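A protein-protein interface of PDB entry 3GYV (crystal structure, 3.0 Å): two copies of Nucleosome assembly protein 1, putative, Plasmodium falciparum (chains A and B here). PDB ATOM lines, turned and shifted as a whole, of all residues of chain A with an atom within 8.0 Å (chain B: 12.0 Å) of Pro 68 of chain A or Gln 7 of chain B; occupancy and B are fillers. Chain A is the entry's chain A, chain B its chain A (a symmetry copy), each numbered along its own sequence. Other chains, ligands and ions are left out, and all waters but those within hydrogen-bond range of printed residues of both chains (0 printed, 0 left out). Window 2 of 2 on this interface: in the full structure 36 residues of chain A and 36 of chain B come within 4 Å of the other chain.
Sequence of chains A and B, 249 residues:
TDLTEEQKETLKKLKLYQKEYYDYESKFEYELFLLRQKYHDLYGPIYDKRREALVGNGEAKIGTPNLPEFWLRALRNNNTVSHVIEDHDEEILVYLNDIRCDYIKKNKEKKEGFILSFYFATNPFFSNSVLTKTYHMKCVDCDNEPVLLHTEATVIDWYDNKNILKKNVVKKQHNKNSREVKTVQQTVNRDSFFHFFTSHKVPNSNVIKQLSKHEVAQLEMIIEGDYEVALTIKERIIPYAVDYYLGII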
ATOM      1  N   ALA A  53     -17.111  25.177   2.287  1.00  0.00           N
ATOM      2  CA  ALA A  53     -15.780  25.222   1.703  1.00  0.00           C
ATOM      3  C   ALA A  53     -15.479  26.505   0.944  1.00  0.00           C
ATOM      4  O   ALA A  53     -14.397  27.055   1.099  1.00  0.00           O
ATOM      5  CB  ALA A  53     -15.560  24.032   0.819  1.00  0.00           C
ATOM      6  N   LEU A  54     -16.429  26.976   0.139  1.00  0.00           N
ATOM      7  CA  LEU A  54     -16.225  28.131  -0.758  1.00  0.00           C
ATOM      8  C   LEU A  54     -16.314  29.461  -0.041  1.00  0.00           C
ATOM      9  O   LEU A  54     -15.454  30.337  -0.214  1.00  0.00           O
ATOM     10  CB  LEU A  54     -17.264  28.137  -1.882  1.00  0.00           C
ATOM     11  CG  LEU A  54     -17.270  27.077  -2.981  1.00  0.00           C
ATOM     12  CD1 LEU A  54     -18.649  27.078  -3.611  1.00  0.00           C
ATOM     13  CD2 LEU A  54     -16.186  27.328  -4.010  1.00  0.00           C
ATOM     14  N   ILE A  62     -16.266  39.638  -0.909  1.00  0.00           N
ATOM     15  CA  ILE A  62     -16.261  39.079  -2.255  1.00  0.00           C
ATOM     16  C   ILE A  62     -16.898  37.683  -2.161  1.00  0.00           C
ATOM     17  O   ILE A  62     -16.805  37.022  -1.132  1.00  0.00           O
ATOM     18  CB  ILE A  62     -14.829  39.109  -2.903  1.00  0.00           C
ATOM     19  CG1 ILE A  62     -14.888  38.894  -4.424  1.00  0.00           C
ATOM     20  CG2 ILE A  62     -13.882  38.119  -2.253  1.00  0.00           C
ATOM     21  CD1 ILE A  62     -15.697  39.949  -5.217  1.00  0.00           C
ATOM     22  N   GLY A  63     -17.601  37.258  -3.199  1.00  0.00           N
ATOM     23  CA  GLY A  63     -18.297  35.972  -3.158  1.00  0.00           C
ATOM     24  C   GLY A  63     -17.328  34.824  -3.329  1.00  0.00           C
ATOM     25  O   GLY A  63     -16.311  34.962  -4.032  1.00  0.00           O
ATOM     26  N   THR A  64     -17.652  33.693  -2.701  1.00  0.00           N
ATOM     27  CA  THR A  64     -16.815  32.473  -2.730  1.00  0.00           C
ATOM     28  C   THR A  64     -15.324  32.772  -2.594  1.00  0.00           C
ATOM     29  O   THR A  64     -14.573  32.527  -3.539  1.00  0.00           O
ATOM     30  CB  THR A  64     -17.041  31.607  -4.005  1.00  0.00           C
ATOM     31  OG1 THR A  64     -17.022  32.438  -5.175  1.00  0.00           O
ATOM     32  CG2 THR A  64     -18.364  30.867  -3.936  1.00  0.00           C
ATOM     33  N   PRO A  65     -14.893  33.303  -1.420  1.00  0.00           N
ATOM     34  CA  PRO A  65     -13.515  33.798  -1.249  1.00  0.00           C
ATOM     35  C   PRO A  65     -12.463  32.706  -1.338  1.00  0.00           C
ATOM     36  O   PRO A  65     -11.365  32.955  -1.824  1.00  0.00           O
ATOM     37  CB  PRO A  65     -13.525  34.414   0.152  1.00  0.00           C
ATOM     38  CG  PRO A  65     -14.933  34.568   0.502  1.00  0.00           C
ATOM     39  CD  PRO A  65     -15.670  33.481  -0.181  1.00  0.00           C
ATOM     40  N   ASN A  66     -12.807  31.500  -0.909  1.00  0.00           N
ATOM     41  CA  ASN A  66     -11.874  30.381  -0.977  1.00  0.00           C
ATOM     42  C   ASN A  66     -11.641  29.797  -2.384  1.00  0.00           C
ATOM     43  O   ASN A  66     -10.803  28.915  -2.560  1.00  0.00           O
ATOM     44  CB  ASN A  66     -12.268  29.309   0.035  1.00  0.00           C
ATOM     45  CG  ASN A  66     -12.261  29.836   1.458  1.00  0.00           C
ATOM     46  OD1 ASN A  66     -11.750  30.927   1.722  1.00  0.00           O
ATOM     47  ND2 ASN A  66     -12.833  29.067   2.385  1.00  0.00           N
ATOM     48  N   LEU A  67     -12.381  30.304  -3.369  1.00  0.00           N
ATOM     49  CA  LEU A  67     -12.169  29.993  -4.778  1.00  0.00           C
ATOM     50  C   LEU A  67     -12.910  31.043  -5.597  1.00  0.00           C
ATOM     51  O   LEU A  67     -13.986  30.778  -6.131  1.00  0.00           O
ATOM     52  CB  LEU A  67     -12.641  28.572  -5.132  1.00  0.00           C
ATOM     53  CG  LEU A  67     -12.086  27.977  -6.438  1.00  0.00           C
ATOM     54  CD1 LEU A  67     -10.706  27.397  -6.229  1.00  0.00           C
ATOM     55  CD2 LEU A  67     -12.985  26.907  -6.951  1.00  0.00           C
ATOM     56  N   PRO A  68     -12.332  32.253  -5.689  1.00  0.00           N
ATOM     57  CA  PRO A  68     -13.019  33.398  -6.273  1.00  0.00           C
ATOM     58  C   PRO A  68     -13.643  33.111  -7.618  1.00  0.00           C
ATOM     59  O   PRO A  68     -13.120  32.304  -8.381  1.00  0.00           O
ATOM     60  CB  PRO A  68     -11.901  34.440  -6.408  1.00  0.00           C
ATOM     61  CG  PRO A  68     -11.004  34.138  -5.278  1.00  0.00           C
ATOM     62  CD  PRO A  68     -10.975  32.627  -5.236  1.00  0.00           C
ATOM     63  N   GLU A  69     -14.754  33.794  -7.880  1.00  0.00           N
ATOM     64  CA  GLU A  69     -15.484  33.753  -9.151  1.00  0.00           C
ATOM     65  C   GLU A  69     -16.134  32.388  -9.465  1.00  0.00           C
ATOM     66  O   GLU A  69     -16.504  32.116 -10.616  1.00  0.00           O
ATOM     67  CB  GLU A  69     -14.591  34.233 -10.299  1.00  0.00           C
ATOM     68  CG  GLU A  69     -13.577  35.286  -9.888  1.00  0.00           C
ATOM     69  CD  GLU A  69     -13.248  36.270 -10.991  1.00  0.00           C
ATOM     70  OE1 GLU A  69     -13.323  35.901 -12.192  1.00  0.00           O
ATOM     71  OE2 GLU A  69     -12.913  37.428 -10.642  1.00  0.00           O
ATOM     72  N   PHE A  70     -16.313  31.559  -8.438  1.00  0.00           N
ATOM     73  CA  PHE A  70     -16.805  30.187  -8.625  1.00  0.00           C
ATOM     74  C   PHE A  70     -18.082  30.082  -9.459  1.00  0.00           C
ATOM     75  O   PHE A  70     -18.032  29.680 -10.615  1.00  0.00           O
ATOM     76  CB  PHE A  70     -16.984  29.445  -7.289  1.00  0.00           C
ATOM     77  CG  PHE A  70     -17.409  28.011  -7.455  1.00  0.00           C
ATOM     78  CD1 PHE A  70     -16.532  27.070  -7.975  1.00  0.00           C
ATOM     79  CD2 PHE A  70     -18.695  27.602  -7.112  1.00  0.00           C
ATOM     80  CE1 PHE A  70     -16.920  25.758  -8.134  1.00  0.00           C
ATOM     81  CE2 PHE A  70     -19.090  26.271  -7.267  1.00  0.00           C
ATOM     82  CZ  PHE A  70     -18.198  25.355  -7.780  1.00  0.00           C
ATOM     83  N   TRP A  71     -19.212  30.437  -8.852  1.00  0.00           N
ATOM     84  CA  TRP A  71     -20.521  30.389  -9.496  1.00  0.00           C
ATOM     85  C   TRP A  71     -20.544  31.088 -10.860  1.00  0.00           C
ATOM     86  O   TRP A  71     -21.193  30.625 -11.792  1.00  0.00           O
ATOM     87  CB  TRP A  71     -21.587  30.955  -8.561  1.00  0.00           C
ATOM     88  CG  TRP A  71     -21.695  30.165  -7.296  1.00  0.00           C
ATOM     89  CD1 TRP A  71     -21.250  30.535  -6.057  1.00  0.00           C
ATOM     90  CD2 TRP A  71     -22.263  28.853  -7.143  1.00  0.00           C
ATOM     91  NE1 TRP A  71     -21.514  29.544  -5.139  1.00  0.00           N
ATOM     92  CE2 TRP A  71     -22.135  28.500  -5.774  1.00  0.00           C
ATOM     93  CE3 TRP A  71     -22.882  27.943  -8.025  1.00  0.00           C
ATOM     94  CZ2 TRP A  71     -22.597  27.275  -5.263  1.00  0.00           C
ATOM     95  CZ3 TRP A  71     -23.347  26.718  -7.510  1.00  0.00           C
ATOM     96  CH2 TRP A  71     -23.196  26.403  -6.139  1.00  0.00           C
ATOM     97  N   LEU A  72     -19.813  32.184 -10.986  1.00  0.00           N
ATOM     98  CA  LEU A  72     -19.711  32.834 -12.269  1.00  0.00           C
ATOM     99  C   LEU A  72     -19.203  31.860 -13.361  1.00  0.00           C
ATOM    100  O   LEU A  72     -19.899  31.622 -14.351  1.00  0.00           O
ATOM    101  CB  LEU A  72     -18.862  34.109 -12.181  1.00  0.00           C
ATOM    102  CG  LEU A  72     -18.610  34.819 -13.521  1.00  0.00           C
ATOM    103  CD1 LEU A  72     -19.921  35.144 -14.261  1.00  0.00           C
ATOM    104  CD2 LEU A  72     -17.774  36.074 -13.333  1.00  0.00           C
ATOM    105  N   ARG A  73     -18.013  31.293 -13.184  1.00  0.00           N
ATOM    106  CA  ARG A  73     -17.460  30.391 -14.202  1.00  0.00           C
ATOM    107  C   ARG A  73     -18.350  29.158 -14.443  1.00  0.00           C
ATOM    108  O   ARG A  73     -18.626  28.795 -15.590  1.00  0.00           O
ATOM    109  CB  ARG A  73     -16.018  30.024 -13.863  1.00  0.00           C
ATOM    110  CG  ARG A  73     -15.137  31.273 -13.736  1.00  0.00           C
ATOM    111  CD  ARG A  73     -13.785  31.020 -13.082  1.00  0.00           C
ATOM    112  NE  ARG A  73     -12.965  32.232 -13.176  1.00  0.00           N
ATOM    113  CZ  ARG A  73     -11.886  32.509 -12.436  1.00  0.00           C
ATOM    114  NH1 ARG A  73     -11.454  31.649 -11.507  1.00  0.00           N
ATOM    115  NH2 ARG A  73     -11.239  33.666 -12.626  1.00  0.00           N
ATOM    116  N   LEU A  93     -21.946  39.163 -10.297  1.00  0.00           N
ATOM    117  CA  LEU A  93     -22.021  37.727 -10.048  1.00  0.00           C
ATOM    118  C   LEU A  93     -20.812  37.197  -9.263  1.00  0.00           C
ATOM    119  O   LEU A  93     -20.936  36.213  -8.531  1.00  0.00           O
ATOM    120  CB  LEU A  93     -22.290  36.950 -11.348  1.00  0.00           C
ATOM    121  CG  LEU A  93     -23.714  37.151 -11.893  1.00  0.00           C
ATOM    122  CD1 LEU A  93     -23.836  36.785 -13.361  1.00  0.00           C
ATOM    123  CD2 LEU A  93     -24.761  36.412 -11.036  1.00  0.00           C
ATOM    124  N   VAL A  94     -19.674  37.881  -9.384  1.00  0.00           N
ATOM    125  CA  VAL A  94     -18.463  37.580  -8.612  1.00  0.00           C
ATOM    126  C   VAL A  94     -18.662  37.648  -7.076  1.00  0.00           C
ATOM    127  O   VAL A  94     -17.775  37.228  -6.295  1.00  0.00           O
ATOM    128  CB  VAL A  94     -17.330  38.551  -8.999  1.00  0.00           C
ATOM    129  CG1 VAL A  94     -16.749  38.195 -10.377  1.00  0.00           C
ATOM    130  CG2 VAL A  94     -17.821  39.976  -8.948  1.00  0.00           C
ATOM    131  N   LEU A  96     -21.555  36.419  -5.738  1.00  0.00           N
ATOM    132  CA  LEU A  96     -22.477  35.347  -5.446  1.00  0.00           C
ATOM    133  C   LEU A  96     -21.787  34.339  -4.541  1.00  0.00           C
ATOM    134  O   LEU A  96     -20.714  33.832  -4.879  1.00  0.00           O
ATOM    135  CB  LEU A  96     -22.885  34.701  -6.760  1.00  0.00           C
ATOM    136  CG  LEU A  96     -24.116  33.812  -6.886  1.00  0.00           C
ATOM    137  CD1 LEU A  96     -25.352  34.403  -6.187  1.00  0.00           C
ATOM    138  CD2 LEU A  96     -24.350  33.613  -8.369  1.00  0.00           C
ATOM    139  N   TYR A 245     -17.624  24.639 -13.690  1.00  0.00           N
ATOM    140  CA  TYR A 245     -16.502  25.485 -13.321  1.00  0.00           C
ATOM    141  C   TYR A 245     -15.194  25.007 -13.948  1.00  0.00           C
ATOM    142  O   TYR A 245     -14.426  25.809 -14.473  1.00  0.00           O
ATOM    143  CB  TYR A 245     -16.378  25.524 -11.795  1.00  0.00           C
ATOM    144  CG  TYR A 245     -15.122  26.199 -11.301  1.00  0.00           C
ATOM    145  CD1 TYR A 245     -15.117  27.570 -10.994  1.00  0.00           C
ATOM    146  CD2 TYR A 245     -13.927  25.473 -11.154  1.00  0.00           C
ATOM    147  CE1 TYR A 245     -13.951  28.197 -10.548  1.00  0.00           C
ATOM    148  CE2 TYR A 245     -12.757  26.088 -10.710  1.00  0.00           C
ATOM    149  CZ  TYR A 245     -12.774  27.442 -10.410  1.00  0.00           C
ATOM    150  OH  TYR A 245     -11.623  28.042  -9.961  1.00  0.00           O
ATOM    151  N   THR B   4      -3.717  29.208  -6.897  1.00  0.00           N
ATOM    152  CA  THR B   4      -3.019  29.192  -5.563  1.00  0.00           C
ATOM    153  C   THR B   4      -3.348  27.924  -4.768  1.00  0.00           C
ATOM    154  O   THR B   4      -4.394  27.308  -4.983  1.00  0.00           O
ATOM    155  CB  THR B   4      -3.372  30.421  -4.696  1.00  0.00           C
ATOM    156  OG1 THR B   4      -4.740  30.341  -4.276  1.00  0.00           O
ATOM    157  CG2 THR B   4      -3.152  31.725  -5.468  1.00  0.00           C
ATOM    158  N   GLU B   5      -2.469  27.545  -3.841  1.00  0.00           N
ATOM    159  CA  GLU B   5      -2.559  26.217  -3.189  1.00  0.00           C
ATOM    160  C   GLU B   5      -3.777  26.145  -2.260  1.00  0.00           C
ATOM    161  O   GLU B   5      -4.409  25.091  -2.089  1.00  0.00           O
ATOM    162  CB  GLU B   5      -1.253  25.805  -2.438  1.00  0.00           C
ATOM    163  CG  GLU B   5       0.138  26.284  -3.013  1.00  0.00           C
ATOM    164  CD  GLU B   5       0.273  26.232  -4.549  1.00  0.00           C
ATOM    165  OE1 GLU B   5      -0.204  25.253  -5.188  1.00  0.00           O
ATOM    166  OE2 GLU B   5       0.868  27.186  -5.116  1.00  0.00           O
ATOM    167  N   GLU B   6      -4.118  27.289  -1.689  1.00  0.00           N
ATOM    168  CA  GLU B   6      -5.241  27.367  -0.784  1.00  0.00           C
ATOM    169  C   GLU B   6      -6.549  27.188  -1.545  1.00  0.00           C
ATOM    170  O   GLU B   6      -7.434  26.466  -1.099  1.00  0.00           O
ATOM    171  CB  GLU B   6      -5.202  28.696  -0.066  1.00  0.00           C
ATOM    172  CG  GLU B   6      -5.652  28.615   1.357  1.00  0.00           C
ATOM    173  CD  GLU B   6      -5.929  29.984   1.903  1.00  0.00           C
ATOM    174  OE1 GLU B   6      -6.939  30.145   2.627  1.00  0.00           O
ATOM    175  OE2 GLU B   6      -5.145  30.905   1.570  1.00  0.00           O
ATOM    176  N   GLN B   7      -6.650  27.849  -2.695  1.00  0.00           N
ATOM    177  CA  GLN B   7      -7.722  27.596  -3.653  1.00  0.00           C
ATOM    178  C   GLN B   7      -7.731  26.141  -4.159  1.00  0.00           C
ATOM    179  O   GLN B   7      -8.777  25.500  -4.231  1.00  0.00           O
ATOM    180  CB  GLN B   7      -7.613  28.573  -4.819  1.00  0.00           C
ATOM    181  CG  GLN B   7      -7.850  30.036  -4.415  1.00  0.00           C
ATOM    182  CD  GLN B   7      -7.423  31.042  -5.485  1.00  0.00           C
ATOM    183  OE1 GLN B   7      -7.243  30.695  -6.655  1.00  0.00           O
ATOM    184  NE2 GLN B   7      -7.263  32.301  -5.076  1.00  0.00           N
ATOM    185  N   LYS B   8      -6.553  25.620  -4.486  1.00  0.00           N
ATOM    186  CA  LYS B   8      -6.395  24.220  -4.873  1.00  0.00           C
ATOM    187  C   LYS B   8      -6.886  23.234  -3.815  1.00  0.00           C
ATOM    188  O   LYS B   8      -7.508  22.235  -4.160  1.00  0.00           O
ATOM    189  CB  LYS B   8      -4.939  23.924  -5.233  1.00  0.00           C
ATOM    190  CG  LYS B   8      -4.545  24.354  -6.649  1.00  0.00           C
ATOM    191  CD  LYS B   8      -3.043  24.161  -6.878  1.00  0.00           C
ATOM    192  CE  LYS B   8      -2.556  24.861  -8.143  1.00  0.00           C
ATOM    193  NZ  LYS B   8      -1.070  24.946  -8.175  1.00  0.00           N
ATOM    194  N   GLU B   9      -6.605  23.499  -2.539  1.00  0.00           N
ATOM    195  CA  GLU B   9      -7.144  22.674  -1.454  1.00  0.00           C
ATOM    196  C   GLU B   9      -8.681  22.729  -1.400  1.00  0.00           C
ATOM    197  O   GLU B   9      -9.343  21.715  -1.157  1.00  0.00           O
ATOM    198  CB  GLU B   9      -6.555  23.078  -0.105  1.00  0.00           C
ATOM    199  CG  GLU B   9      -5.519  22.127   0.466  1.00  0.00           C
ATOM    200  CD  GLU B   9      -6.040  20.700   0.714  1.00  0.00           C
ATOM    201  OE1 GLU B   9      -7.260  20.504   0.983  1.00  0.00           O
ATOM    202  OE2 GLU B   9      -5.202  19.758   0.651  1.00  0.00           O
ATOM    203  N   THR B  10      -9.248  23.909  -1.631  1.00  0.00           N
ATOM    204  CA  THR B  10     -10.687  24.033  -1.738  1.00  0.00           C
ATOM    205  C   THR B  10     -11.218  23.133  -2.857  1.00  0.00           C
ATOM    206  O   THR B  10     -12.178  22.388  -2.666  1.00  0.00           O
ATOM    207  CB  THR B  10     -11.120  25.493  -1.973  1.00  0.00           C
ATOM    208  OG1 THR B  10     -11.044  26.214  -0.741  1.00  0.00           O
ATOM    209  CG2 THR B  10     -12.537  25.548  -2.453  1.00  0.00           C
ATOM    210  N   LEU B  11     -10.569  23.194  -4.016  1.00  0.00           N
ATOM    211  CA  LEU B  11     -11.025  22.488  -5.202  1.00  0.00           C
ATOM    212  C   LEU B  11     -10.986  20.977  -5.037  1.00  0.00           C
ATOM    213  O   LEU B  11     -11.846  20.286  -5.578  1.00  0.00           O
ATOM    214  CB  LEU B  11     -10.207  22.926  -6.409  1.00  0.00           C
ATOM    215  CG  LEU B  11     -10.641  22.478  -7.801  1.00  0.00           C
ATOM    216  CD1 LEU B  11     -11.993  23.059  -8.159  1.00  0.00           C
ATOM    217  CD2 LEU B  11      -9.595  22.892  -8.836  1.00  0.00           C
ATOM    218  N   LYS B  12     -10.007  20.465  -4.286  1.00  0.00           N
ATOM    219  CA  LYS B  12      -9.945  19.022  -4.002  1.00  0.00           C
ATOM    220  C   LYS B  12     -11.178  18.639  -3.243  1.00  0.00           C
ATOM    221  O   LYS B  12     -11.856  17.695  -3.618  1.00  0.00           O
ATOM    222  CB  LYS B  12      -8.692  18.593  -3.217  1.00  0.00           C
ATOM    223  CG  LYS B  12      -7.391  18.898  -3.955  1.00  0.00           C
ATOM    224  CD  LYS B  12      -6.390  17.738  -3.976  1.00  0.00           C
ATOM    225  CE  LYS B  12      -4.998  18.189  -4.520  1.00  0.00           C
ATOM    226  NZ  LYS B  12      -4.757  18.052  -5.989  1.00  0.00           N
ATOM    227  N   LYS B  13     -11.479  19.398  -2.195  1.00  0.00           N
ATOM    228  CA  LYS B  13     -12.674  19.166  -1.396  1.00  0.00           C
ATOM    229  C   LYS B  13     -13.944  19.167  -2.254  1.00  0.00           C
ATOM    230  O   LYS B  13     -14.780  18.280  -2.130  1.00  0.00           O
ATOM    231  CB  LYS B  13     -12.772  20.207  -0.284  1.00  0.00           C
ATOM    232  CG  LYS B  13     -11.500  20.340   0.551  1.00  0.00           C
ATOM    233  CD  LYS B  13     -11.624  21.461   1.577  1.00  0.00           C
ATOM    234  CE  LYS B  13     -12.393  20.992   2.802  1.00  0.00           C
ATOM    235  NZ  LYS B  13     -13.109  22.118   3.499  1.00  0.00           N
ATOM    236  N   LEU B  14     -14.062  20.147  -3.144  1.00  0.00           N
ATOM    237  CA  LEU B  14     -15.213  20.250  -4.054  1.00  0.00           C
ATOM    238  C   LEU B  14     -15.370  19.085  -5.041  1.00  0.00           C
ATOM    239  O   LEU B  14     -16.495  18.662  -5.306  1.00  0.00           O
ATOM    240  CB  LEU B  14     -15.212  21.589  -4.799  1.00  0.00           C
ATOM    241  CG  LEU B  14     -16.056  22.727  -4.212  1.00  0.00           C
ATOM    242  CD1 LEU B  14     -15.603  23.157  -2.830  1.00  0.00           C
ATOM    243  CD2 LEU B  14     -16.025  23.901  -5.163  1.00  0.00           C
ATOM    244  N   LYS B  15     -14.255  18.578  -5.577  1.00  0.00           N
ATOM    245  CA  LYS B  15     -14.255  17.330  -6.361  1.00  0.00           C
ATOM    246  C   LYS B  15     -14.701  16.160  -5.498  1.00  0.00           C
ATOM    247  O   LYS B  15     -15.449  15.295  -5.957  1.00  0.00           O
ATOM    248  CB  LYS B  15     -12.871  17.019  -6.924  1.00  0.00           C
ATOM    249  CG  LYS B  15     -12.415  17.950  -8.019  1.00  0.00           C
ATOM    250  CD  LYS B  15     -10.938  17.720  -8.355  1.00  0.00           C
ATOM    251  CE  LYS B  15     -10.425  18.723  -9.360  1.00  0.00           C
ATOM    252  NZ  LYS B  15      -9.086  18.314  -9.769  1.00  0.00           N
ATOM    253  N   LEU B  16     -14.239  16.139  -4.248  1.00  0.00           N
ATOM    254  CA  LEU B  16     -14.603  15.076  -3.329  1.00  0.00           C
ATOM    255  C   LEU B  16     -16.107  15.061  -3.123  1.00  0.00           C
ATOM    256  O   LEU B  16     -16.753  14.018  -3.266  1.00  0.00           O
ATOM    257  CB  LEU B  16     -13.906  15.216  -1.977  1.00  0.00           C
ATOM    258  CG  LEU B  16     -13.947  13.871  -1.249  1.00  0.00           C
ATOM    259  CD1 LEU B  16     -12.556  13.226  -1.275  1.00  0.00           C
ATOM    260  CD2 LEU B  16     -14.474  14.014   0.172  1.00  0.00           C
ATOM    261  N   TYR B  17     -16.669  16.222  -2.814  1.00  0.00           N
ATOM    262  CA  TYR B  17     -18.092  16.297  -2.569  1.00  0.00           C
ATOM    263  C   TYR B  17     -18.926  16.021  -3.828  1.00  0.00           C
ATOM    264  O   TYR B  17     -20.073  15.609  -3.719  1.00  0.00           O
ATOM    265  CB  TYR B  17     -18.474  17.636  -1.956  1.00  0.00           C
ATOM    266  CG  TYR B  17     -17.642  18.095  -0.776  1.00  0.00           C
ATOM    267  CD1 TYR B  17     -17.168  17.195   0.185  1.00  0.00           C
ATOM    268  CD2 TYR B  17     -17.367  19.451  -0.602  1.00  0.00           C
ATOM    269  CE1 TYR B  17     -16.409  17.635   1.260  1.00  0.00           C
ATOM    270  CE2 TYR B  17     -16.626  19.902   0.471  1.00  0.00           C
ATOM    271  CZ  TYR B  17     -16.150  18.995   1.400  1.00  0.00           C
ATOM    272  OH  TYR B  17     -15.410  19.477   2.462  1.00  0.00           O
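The side-chain amide nitrogen (NE2) of Gln 7 of chain B sits close to the side-chain hydroxyl (OG1) of Thr 4 of chain B (3.3 Å). The backbone NH (N) of Phe 70 of chain A sits at hydrogen-bond distance from the side-chain hydroxyl (OG1) of Thr 64 of chain A (3.5 Å). The backbone NH of Asn 66 of chain A sits at hydrogen-bond distance from the backbone carbonyl oxygen of Leu 54 of chain A, 3.0 Å away. O of Ala 53 of chain A sits at hydrogen-bond distance from ND2 of Asn 66 of chain A (2.9 Å).
Of chain B, only Gln 7 (3.7 Å) comes within 4 Å of Pro 68 of chain A. Of the printed residues of chain A, Gln 7 of chain B touches Asn 66, Leu 67 and Pro 68. No residue of chain B comes within 4 Å of Gly 63 of chain A. No residue of chain B comes within 4 Å of Thr 64 of chain A. Of chain B, only Gln 7 (3.4 Å) comes within 4 Å of Leu 67 of chain A. Of the printed residues of chain B, Ala 53 of chain A touches Thr 10 (3.9 Å) and Leu 14 (3.8 Å). Of the printed residues of chain B, Phe 70 of chain A touches Leu 14 (3.6 Å). The nearest residue of chain B that does not touch Pro 68 of chain A is Thr 4 of chain B (6.7 Å). The nearest residue of chain A that does not touch Gln 7 of chain B is Pro 65 of chain A (5.3 Å). The nearest printed residue of chain A that does not touch Thr 10 of chain B is Leu 67 of chain A (4.04 Å).
Among the printed residues, pairs that only touch across the chains: Ala 53 of chain A with Thr 10 of chain B, Ala 53 of chain A with Leu 14 of chain B, Leu 54 of chain A with Leu 14 of chain B, Asn 66 of chain A with Gln 7 of chain B, Leu 67 of chain A with Gln 7 of chain B, Pro 68 of chain A with Gln 7 of chain B and Phe 70 of chain A with Leu 14 of chain B.
The backbone carbonyl oxygen of Asn 66 of chain A lies within hydrogen-bond range of the side-chain hydroxyl of Thr 10 of chain B.
No position is printed for both chains. Of the 8 pairs that touch across the chains among the printed residues, none has its exchanged pair printed and touching as well.
Of the 14 printed residues of chain B, 3 touch a printed residue of chain A. Printed residues of chain B that touch a printed residue of chain A: Gln 7, Thr 10 and Leu 14. Hydrophobic or aromatic side chains of chain B that line the printed part of chain A: Leu 14. Among the printed residues, 8 pairs touch across the chains.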
